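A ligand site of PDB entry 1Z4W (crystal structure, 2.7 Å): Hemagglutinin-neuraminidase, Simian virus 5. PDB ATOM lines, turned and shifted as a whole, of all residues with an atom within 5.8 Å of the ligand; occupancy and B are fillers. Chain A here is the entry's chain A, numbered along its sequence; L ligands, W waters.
OH of Tyr 273 is in hydrogen-bond range of O6 of the ligand, at 3.1 Å.
NH1 of Arg 130 lies within salt-bridge range of O1 of the ligand (2.8 Å).
OH of Tyr 490 lies close to O4 of the ligand, at 3.1 Å.
The guanidinium group (NH2) of Arg 372 lies within salt-bridge range of an oxygen (O2) of the ligand, 3.3 Å away.
An oxygen (O2) of the ligand is in salt-bridge range of the guanidinium group of Arg 462, 2.5 Å away.
OE1 of Glu 214 lies within hydrogen-bond range of O5 of the ligand, at 2.6 Å.
OD1 of Asn 374 is in hydrogen-bond range of N of Gly 428 (3.4 Å).
The side-chain carboxylate (OE1) of Glu 511 lies within hydrogen-bond range of the backbone NH (N) of Tyr 490, at 2.9 Å.
The side-chain carboxylate (OE2) of Glu 511 is in hydrogen-bond range of the backbone NH (N) of Ile 131, at 2.8 Å.
The backbone carbonyl oxygen of Tyr 273 is in hydrogen-bond range of the backbone NH of Asn 255, at 2.8 Å.
NH2 of Arg 130 lies within salt-bridge range of OE1 of Glu 511 (2.9 Å).
OE1 of Glu 357 sits at hydrogen-bond distance from OH of Tyr 490.
The guanidinium group (NH1) of Arg 372 sits at hydrogen-bond distance from the side-chain hydroxyl (OH) of Tyr 490 (2.8 Å).
NH2 of Arg 462 is in hydrogen-bond range of O of Gly 428 (2.8 Å).
CD1 of Ile 131 touches O3 of the ligand (3.7 Å).
CE2 of Phe 208 touches C11 of the ligand, at 3.8 Å.
Asn 255 touches the ligand.
CG of Glu 357 touches O6 of the ligand, 3.5 Å away.
Asn 374 touches the ligand (ND2 to C9, 3.9 Å).
Hydrophobic or aromatic side chains within 4 Å of the ligand: Ile 131, Phe 208, Tyr 273 and Tyr 490.
Of the 21 residues printed, 11 come within 4 Å of the ligand.
The nearest printed residue that does not touch the ligand is Phe 320 (4.1 Å).
Water W2 lies within hydrogen-bond range of an oxygen (O3) of the ligand (2.8 Å) and the backbone NH of Ser 193 (3.2 Å).
Water W1 lies within hydrogen-bond range of an oxygen (O7) of the ligand (2.8 Å) and the side-chain hydroxyl (OH) of Tyr 218 (3.2 Å).
Water W5 bridges an oxygen (O6) of the ligand and the backbone NH of Glu 357.
Water W3 lies within hydrogen-bond range of OH of Tyr 273 (2.7 Å), OE2 of Glu 357 (2.7 Å), OG of Ser 193 (2.8 Å) and N1 of the ligand (2.9 Å).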
ATOM      1  N   ARG A 130     -15.694 -17.767  -9.826  1.00  0.00           N
ATOM      2  CA  ARG A 130     -16.918 -17.168 -10.358  1.00  0.00           C
ATOM      3  C   ARG A 130     -17.171 -17.487 -11.814  1.00  0.00           C
ATOM      4  O   ARG A 130     -16.328 -18.081 -12.480  1.00  0.00           O
ATOM      5  CB  ARG A 130     -16.886 -15.655 -10.232  1.00  0.00           C
ATOM      6  CG  ARG A 130     -17.178 -15.104  -8.855  1.00  0.00           C
ATOM      7  CD  ARG A 130     -17.827 -13.749  -9.009  1.00  0.00           C
ATOM      8  NE  ARG A 130     -19.097 -13.860  -9.740  1.00  0.00           N
ATOM      9  CZ  ARG A 130     -19.788 -12.835 -10.235  1.00  0.00           C
ATOM     10  NH1 ARG A 130     -19.349 -11.600 -10.088  1.00  0.00           N
ATOM     11  NH2 ARG A 130     -20.929 -13.053 -10.874  1.00  0.00           N
ATOM     12  N   ILE A 131     -18.338 -17.066 -12.289  1.00  0.00           N
ATOM     13  CA  ILE A 131     -18.756 -17.230 -13.687  1.00  0.00           C
ATOM     14  C   ILE A 131     -18.757 -18.668 -14.173  1.00  0.00           C
ATOM     15  O   ILE A 131     -17.934 -19.065 -14.994  1.00  0.00           O
ATOM     16  CB  ILE A 131     -17.864 -16.405 -14.626  1.00  0.00           C
ATOM     17  CG1 ILE A 131     -17.548 -15.053 -14.005  1.00  0.00           C
ATOM     18  CG2 ILE A 131     -18.564 -16.206 -15.957  1.00  0.00           C
ATOM     19  CD1 ILE A 131     -18.780 -14.226 -13.678  1.00  0.00           C
ATOM     20  N   LYS A 192     -11.564 -15.142 -20.141  1.00  0.00           N
ATOM     21  CA  LYS A 192     -12.694 -14.683 -19.334  1.00  0.00           C
ATOM     22  C   LYS A 192     -14.057 -14.913 -19.983  1.00  0.00           C
ATOM     23  O   LYS A 192     -14.146 -15.224 -21.170  1.00  0.00           O
ATOM     24  CB  LYS A 192     -12.574 -13.186 -19.047  1.00  0.00           C
ATOM     25  CG  LYS A 192     -11.441 -12.772 -18.124  1.00  0.00           C
ATOM     26  CD  LYS A 192     -11.731 -13.149 -16.691  1.00  0.00           C
ATOM     27  CE  LYS A 192     -10.776 -12.434 -15.744  1.00  0.00           C
ATOM     28  NZ  LYS A 192     -11.016 -12.800 -14.329  1.00  0.00           N
ATOM     29  N   SER A 193     -15.104 -14.762 -19.176  1.00  0.00           N
ATOM     30  CA  SER A 193     -16.481 -14.888 -19.630  1.00  0.00           C
ATOM     31  C   SER A 193     -16.699 -16.111 -20.536  1.00  0.00           C
ATOM     32  O   SER A 193     -17.424 -16.050 -21.518  1.00  0.00           O
ATOM     33  CB  SER A 193     -16.851 -13.590 -20.360  1.00  0.00           C
ATOM     34  OG  SER A 193     -18.225 -13.501 -20.669  1.00  0.00           O
ATOM     35  N   PHE A 208     -12.749 -15.153 -24.325  1.00  0.00           N
ATOM     36  CA  PHE A 208     -12.111 -14.000 -24.932  1.00  0.00           C
ATOM     37  C   PHE A 208     -10.997 -13.656 -23.955  1.00  0.00           C
ATOM     38  O   PHE A 208     -11.144 -13.884 -22.764  1.00  0.00           O
ATOM     39  CB  PHE A 208     -13.116 -12.842 -25.100  1.00  0.00           C
ATOM     40  CG  PHE A 208     -13.246 -11.942 -23.883  1.00  0.00           C
ATOM     41  CD1 PHE A 208     -12.421 -10.834 -23.729  1.00  0.00           C
ATOM     42  CD2 PHE A 208     -14.240 -12.169 -22.942  1.00  0.00           C
ATOM     43  CE1 PHE A 208     -12.581  -9.959 -22.656  1.00  0.00           C
ATOM     44  CE2 PHE A 208     -14.420 -11.301 -21.870  1.00  0.00           C
ATOM     45  CZ  PHE A 208     -13.593 -10.186 -21.723  1.00  0.00           C
ATOM     46  N   GLU A 214     -13.287  -3.968 -18.347  1.00  0.00           N
ATOM     47  CA  GLU A 214     -14.361  -4.163 -19.300  1.00  0.00           C
ATOM     48  C   GLU A 214     -14.704  -2.903 -20.070  1.00  0.00           C
ATOM     49  O   GLU A 214     -14.808  -2.914 -21.292  1.00  0.00           O
ATOM     50  CB  GLU A 214     -15.614  -4.685 -18.582  1.00  0.00           C
ATOM     51  CG  GLU A 214     -16.860  -4.661 -19.465  1.00  0.00           C
ATOM     52  CD  GLU A 214     -18.039  -5.369 -18.845  1.00  0.00           C
ATOM     53  OE1 GLU A 214     -18.297  -5.157 -17.642  1.00  0.00           O
ATOM     54  OE2 GLU A 214     -18.715  -6.143 -19.568  1.00  0.00           O
ATOM     55  N   TYR A 218     -14.891  -1.522 -24.506  1.00  0.00           N
ATOM     56  CA  TYR A 218     -15.885  -0.864 -25.331  1.00  0.00           C
ATOM     57  C   TYR A 218     -15.372   0.390 -26.038  1.00  0.00           C
ATOM     58  O   TYR A 218     -15.795   0.707 -27.150  1.00  0.00           O
ATOM     59  CB  TYR A 218     -17.118  -0.526 -24.500  1.00  0.00           C
ATOM     60  CG  TYR A 218     -17.965  -1.738 -24.178  1.00  0.00           C
ATOM     61  CD1 TYR A 218     -17.648  -2.564 -23.091  1.00  0.00           C
ATOM     62  CD2 TYR A 218     -19.032  -2.115 -24.995  1.00  0.00           C
ATOM     63  CE1 TYR A 218     -18.361  -3.727 -22.841  1.00  0.00           C
ATOM     64  CE2 TYR A 218     -19.754  -3.278 -24.749  1.00  0.00           C
ATOM     65  CZ  TYR A 218     -19.413  -4.080 -23.673  1.00  0.00           C
ATOM     66  OH  TYR A 218     -20.113  -5.249 -23.426  1.00  0.00           O
ATOM     67  N   ASN A 255     -18.029 -10.842 -26.445  1.00  0.00           N
ATOM     68  CA  ASN A 255     -17.879 -11.752 -25.310  1.00  0.00           C
ATOM     69  C   ASN A 255     -18.787 -12.956 -25.384  1.00  0.00           C
ATOM     70  O   ASN A 255     -19.894 -12.876 -25.909  1.00  0.00           O
ATOM     71  CB  ASN A 255     -18.262 -11.060 -23.984  1.00  0.00           C
ATOM     72  CG  ASN A 255     -17.339  -9.929 -23.615  1.00  0.00           C
ATOM     73  OD1 ASN A 255     -16.334  -9.675 -24.282  1.00  0.00           O
ATOM     74  ND2 ASN A 255     -17.680  -9.243 -22.532  1.00  0.00           N
ATOM     75  N   TYR A 273     -22.360 -11.447 -26.918  1.00  0.00           N
ATOM     76  CA  TYR A 273     -22.833 -10.088 -26.752  1.00  0.00           C
ATOM     77  C   TYR A 273     -21.646  -9.151 -26.774  1.00  0.00           C
ATOM     78  O   TYR A 273     -20.507  -9.579 -26.584  1.00  0.00           O
ATOM     79  CB  TYR A 273     -23.653  -9.944 -25.454  1.00  0.00           C
ATOM     80  CG  TYR A 273     -22.867  -9.828 -24.171  1.00  0.00           C
ATOM     81  CD1 TYR A 273     -22.261 -10.943 -23.589  1.00  0.00           C
ATOM     82  CD2 TYR A 273     -22.744  -8.603 -23.515  1.00  0.00           C
ATOM     83  CE1 TYR A 273     -21.561 -10.840 -22.387  1.00  0.00           C
ATOM     84  CE2 TYR A 273     -22.054  -8.486 -22.315  1.00  0.00           C
ATOM     85  CZ  TYR A 273     -21.473  -9.608 -21.751  1.00  0.00           C
ATOM     86  OH  TYR A 273     -20.806  -9.485 -20.551  1.00  0.00           O
ATOM     87  N   PHE A 320     -20.488   2.811 -21.979  1.00  0.00           N
ATOM     88  CA  PHE A 320     -19.693   1.787 -22.632  1.00  0.00           C
ATOM     89  C   PHE A 320     -19.305   2.218 -24.044  1.00  0.00           C
ATOM     90  O   PHE A 320     -19.796   1.676 -25.037  1.00  0.00           O
ATOM     91  CB  PHE A 320     -20.451   0.454 -22.669  1.00  0.00           C
ATOM     92  CG  PHE A 320     -20.239  -0.396 -21.450  1.00  0.00           C
ATOM     93  CD1 PHE A 320     -19.260  -0.055 -20.511  1.00  0.00           C
ATOM     94  CD2 PHE A 320     -20.998  -1.543 -21.247  1.00  0.00           C
ATOM     95  CE1 PHE A 320     -19.048  -0.855 -19.378  1.00  0.00           C
ATOM     96  CE2 PHE A 320     -20.783  -2.349 -20.121  1.00  0.00           C
ATOM     97  CZ  PHE A 320     -19.814  -2.009 -19.185  1.00  0.00           C
ATOM     98  N   ALA A 356     -26.800  -8.742 -23.756  1.00  0.00           N
ATOM     99  CA  ALA A 356     -26.369  -9.128 -22.412  1.00  0.00           C
ATOM    100  C   ALA A 356     -25.856 -10.559 -22.455  1.00  0.00           C
ATOM    101  O   ALA A 356     -25.874 -11.206 -23.497  1.00  0.00           O
ATOM    102  CB  ALA A 356     -27.540  -9.019 -21.451  1.00  0.00           C
ATOM    103  N   GLU A 357     -25.390 -11.041 -21.305  1.00  0.00           N
ATOM    104  CA  GLU A 357     -24.901 -12.407 -21.206  1.00  0.00           C
ATOM    105  C   GLU A 357     -26.101 -13.276 -21.570  1.00  0.00           C
ATOM    106  O   GLU A 357     -27.227 -12.800 -21.575  1.00  0.00           O
ATOM    107  CB  GLU A 357     -24.439 -12.712 -19.780  1.00  0.00           C
ATOM    108  CG  GLU A 357     -23.307 -11.835 -19.296  1.00  0.00           C
ATOM    109  CD  GLU A 357     -22.922 -12.131 -17.868  1.00  0.00           C
ATOM    110  OE1 GLU A 357     -23.832 -12.189 -17.015  1.00  0.00           O
ATOM    111  OE2 GLU A 357     -21.706 -12.291 -17.591  1.00  0.00           O
ATOM    112  N   ARG A 372     -29.941 -12.346 -20.336  1.00  0.00           N
ATOM    113  CA  ARG A 372     -29.864 -11.652 -19.061  1.00  0.00           C
ATOM    114  C   ARG A 372     -30.577 -10.307 -19.218  1.00  0.00           C
ATOM    115  O   ARG A 372     -30.473  -9.641 -20.243  1.00  0.00           O
ATOM    116  CB  ARG A 372     -28.389 -11.436 -18.674  1.00  0.00           C
ATOM    117  CG  ARG A 372     -28.148 -10.435 -17.562  1.00  0.00           C
ATOM    118  CD  ARG A 372     -26.691 -10.439 -17.113  1.00  0.00           C
ATOM    119  NE  ARG A 372     -26.352  -9.254 -16.348  1.00  0.00           N
ATOM    120  CZ  ARG A 372     -25.263  -9.105 -15.599  1.00  0.00           C
ATOM    121  NH1 ARG A 372     -24.386 -10.101 -15.502  1.00  0.00           N
ATOM    122  NH2 ARG A 372     -25.026  -7.972 -14.955  1.00  0.00           N
ATOM    123  N   ASN A 374     -30.268  -7.092 -18.449  1.00  0.00           N
ATOM    124  CA  ASN A 374     -29.319  -6.087 -17.999  1.00  0.00           C
ATOM    125  C   ASN A 374     -29.815  -4.702 -18.411  1.00  0.00           C
ATOM    126  O   ASN A 374     -29.114  -3.711 -18.234  1.00  0.00           O
ATOM    127  CB  ASN A 374     -27.933  -6.355 -18.620  1.00  0.00           C
ATOM    128  CG  ASN A 374     -26.798  -5.969 -17.699  1.00  0.00           C
ATOM    129  OD1 ASN A 374     -26.799  -6.309 -16.516  1.00  0.00           O
ATOM    130  ND2 ASN A 374     -25.823  -5.258 -18.237  1.00  0.00           N
ATOM    131  N   LEU A 426     -28.193  -0.391 -17.363  1.00  0.00           N
ATOM    132  CA  LEU A 426     -27.022  -1.234 -17.532  1.00  0.00           C
ATOM    133  C   LEU A 426     -26.730  -1.856 -16.174  1.00  0.00           C
ATOM    134  O   LEU A 426     -25.677  -1.639 -15.585  1.00  0.00           O
ATOM    135  CB  LEU A 426     -25.832  -0.415 -18.022  1.00  0.00           C
ATOM    136  CG  LEU A 426     -24.597  -1.179 -18.501  1.00  0.00           C
ATOM    137  CD1 LEU A 426     -24.960  -2.053 -19.693  1.00  0.00           C
ATOM    138  CD2 LEU A 426     -23.504  -0.204 -18.890  1.00  0.00           C
ATOM    139  N   GLY A 428     -28.027  -5.492 -13.493  1.00  0.00           N
ATOM    140  CA  GLY A 428     -28.762  -6.738 -13.374  1.00  0.00           C
ATOM    141  C   GLY A 428     -27.873  -7.889 -12.938  1.00  0.00           C
ATOM    142  O   GLY A 428     -26.796  -7.687 -12.409  1.00  0.00           O
ATOM    143  N   VAL A 429     -28.352  -9.122 -13.146  1.00  0.00           N
ATOM    144  CA  VAL A 429     -27.602 -10.324 -12.792  1.00  0.00           C
ATOM    145  C   VAL A 429     -28.029 -11.429 -13.720  1.00  0.00           C
ATOM    146  O   VAL A 429     -29.128 -11.404 -14.264  1.00  0.00           O
ATOM    147  CB  VAL A 429     -27.905 -10.849 -11.372  1.00  0.00           C
ATOM    148  CG1 VAL A 429     -26.640 -10.854 -10.541  1.00  0.00           C
ATOM    149  CG2 VAL A 429     -29.025 -10.050 -10.723  1.00  0.00           C
ATOM    150  N   ARG A 462     -27.787  -7.941  -4.463  1.00  0.00           N
ATOM    151  CA  ARG A 462     -27.617  -9.331  -4.894  1.00  0.00           C
ATOM    152  C   ARG A 462     -27.679 -10.131  -3.608  1.00  0.00           C
ATOM    153  O   ARG A 462     -26.667 -10.573  -3.065  1.00  0.00           O
ATOM    154  CB  ARG A 462     -26.282  -9.494  -5.614  1.00  0.00           C
ATOM    155  CG  ARG A 462     -26.276  -8.798  -6.971  1.00  0.00           C
ATOM    156  CD  ARG A 462     -25.033  -9.133  -7.744  1.00  0.00           C
ATOM    157  NE  ARG A 462     -25.100  -8.653  -9.121  1.00  0.00           N
ATOM    158  CZ  ARG A 462     -24.171  -8.901 -10.030  1.00  0.00           C
ATOM    159  NH1 ARG A 462     -23.090  -9.606  -9.701  1.00  0.00           N
ATOM    160  NH2 ARG A 462     -24.314  -8.444 -11.264  1.00  0.00           N
ATOM    161  N   ALA A 489     -24.933 -14.431  -6.342  1.00  0.00           N
ATOM    162  CA  ALA A 489     -24.806 -13.782  -7.649  1.00  0.00           C
ATOM    163  C   ALA A 489     -25.554 -14.537  -8.741  1.00  0.00           C
ATOM    164  O   ALA A 489     -26.785 -14.617  -8.715  1.00  0.00           O
ATOM    165  CB  ALA A 489     -23.332 -13.620  -8.000  1.00  0.00           C
ATOM    166  N   TYR A 490     -24.810 -15.090  -9.708  1.00  0.00           N
ATOM    167  CA  TYR A 490     -25.405 -15.826 -10.837  1.00  0.00           C
ATOM    168  C   TYR A 490     -26.037 -17.152 -10.451  1.00  0.00           C
ATOM    169  O   TYR A 490     -25.703 -17.744  -9.425  1.00  0.00           O
ATOM    170  CB  TYR A 490     -24.350 -16.126 -11.901  1.00  0.00           C
ATOM    171  CG  TYR A 490     -23.788 -14.944 -12.649  1.00  0.00           C
ATOM    172  CD1 TYR A 490     -24.086 -13.635 -12.268  1.00  0.00           C
ATOM    173  CD2 TYR A 490     -22.949 -15.132 -13.746  1.00  0.00           C
ATOM    174  CE1 TYR A 490     -23.561 -12.538 -12.971  1.00  0.00           C
ATOM    175  CE2 TYR A 490     -22.425 -14.057 -14.443  1.00  0.00           C
ATOM    176  CZ  TYR A 490     -22.733 -12.770 -14.062  1.00  0.00           C
ATOM    177  OH  TYR A 490     -22.224 -11.729 -14.776  1.00  0.00           O
ATOM    178  N   GLU A 511     -23.953 -19.024  -7.276  1.00  0.00           N
ATOM    179  CA  GLU A 511     -22.754 -18.442  -6.698  1.00  0.00           C
ATOM    180  C   GLU A 511     -23.118 -17.902  -5.327  1.00  0.00           C
ATOM    181  O   GLU A 511     -23.818 -16.899  -5.218  1.00  0.00           O
ATOM    182  CB  GLU A 511     -22.223 -17.311  -7.555  1.00  0.00           C
ATOM    183  CG  GLU A 511     -21.753 -17.717  -8.932  1.00  0.00           C
ATOM    184  CD  GLU A 511     -21.182 -16.540  -9.700  1.00  0.00           C
ATOM    185  OE1 GLU A 511     -21.921 -15.585  -9.984  1.00  0.00           O
ATOM    186  OE2 GLU A 511     -19.975 -16.574 -10.014  1.00  0.00           O
HETATM  187  C1  LIG L   1     -21.474  -9.528 -12.870  1.00  0.00           C
HETATM  188  C2  LIG L   1     -20.581  -9.637 -13.945  1.00  0.00           C
HETATM  189  C3  LIG L   1     -19.372 -10.540 -13.877  1.00  0.00           C
HETATM  190  C4  LIG L   1     -18.706 -10.773 -15.244  1.00  0.00           C
HETATM  191  C5  LIG L   1     -18.794  -9.533 -16.116  1.00  0.00           C
HETATM  192  C6  LIG L   1     -20.282  -9.196 -16.312  1.00  0.00           C
HETATM  193  C7  LIG L   1     -20.467  -7.935 -17.158  1.00  0.00           C
HETATM  194  C8  LIG L   1     -21.928  -7.584 -17.426  1.00  0.00           C
HETATM  195  C9  LIG L   1     -22.084  -6.301 -18.266  1.00  0.00           C
HETATM  196  C10 LIG L   1     -17.095  -9.211 -17.885  1.00  0.00           C
HETATM  197  C11 LIG L   1     -16.544  -9.645 -19.218  1.00  0.00           C
HETATM  198  N1  LIG L   1     -18.150  -9.859 -17.394  1.00  0.00           N
HETATM  199  O1  LIG L   1     -21.227 -10.149 -11.644  1.00  0.00           O
HETATM  200  O2  LIG L   1     -22.563  -8.849 -12.983  1.00  0.00           O
HETATM  201  O3  LIG L   1     -17.345 -11.133 -15.023  1.00  0.00           O
HETATM  202  O4  LIG L   1     -20.879  -8.933 -15.015  1.00  0.00           O
HETATM  203  O5  LIG L   1     -19.934  -6.803 -16.475  1.00  0.00           O
HETATM  204  O6  LIG L   1     -22.536  -8.668 -18.140  1.00  0.00           O
HETATM  205  O7  LIG L   1     -21.421  -6.338 -19.499  1.00  0.00           O
HETATM  206  O8  LIG L   1     -16.486  -8.158 -17.227  1.00  0.00           O
HETATM  207  O   HOH W   1     -22.845  -5.208 -21.675  1.00  0.00           O
HETATM  208  O   HOH W   2     -16.111 -12.455 -17.175  1.00  0.00           O
HETATM  209  O   HOH W   3     -19.634 -11.555 -19.211  1.00  0.00           O
HETATM  210  O   HOH W   4     -13.736  -7.981 -17.989  1.00  0.00           O
HETATM  211  O   HOH W   5     -25.001  -8.602 -19.589  1.00  0.00           O
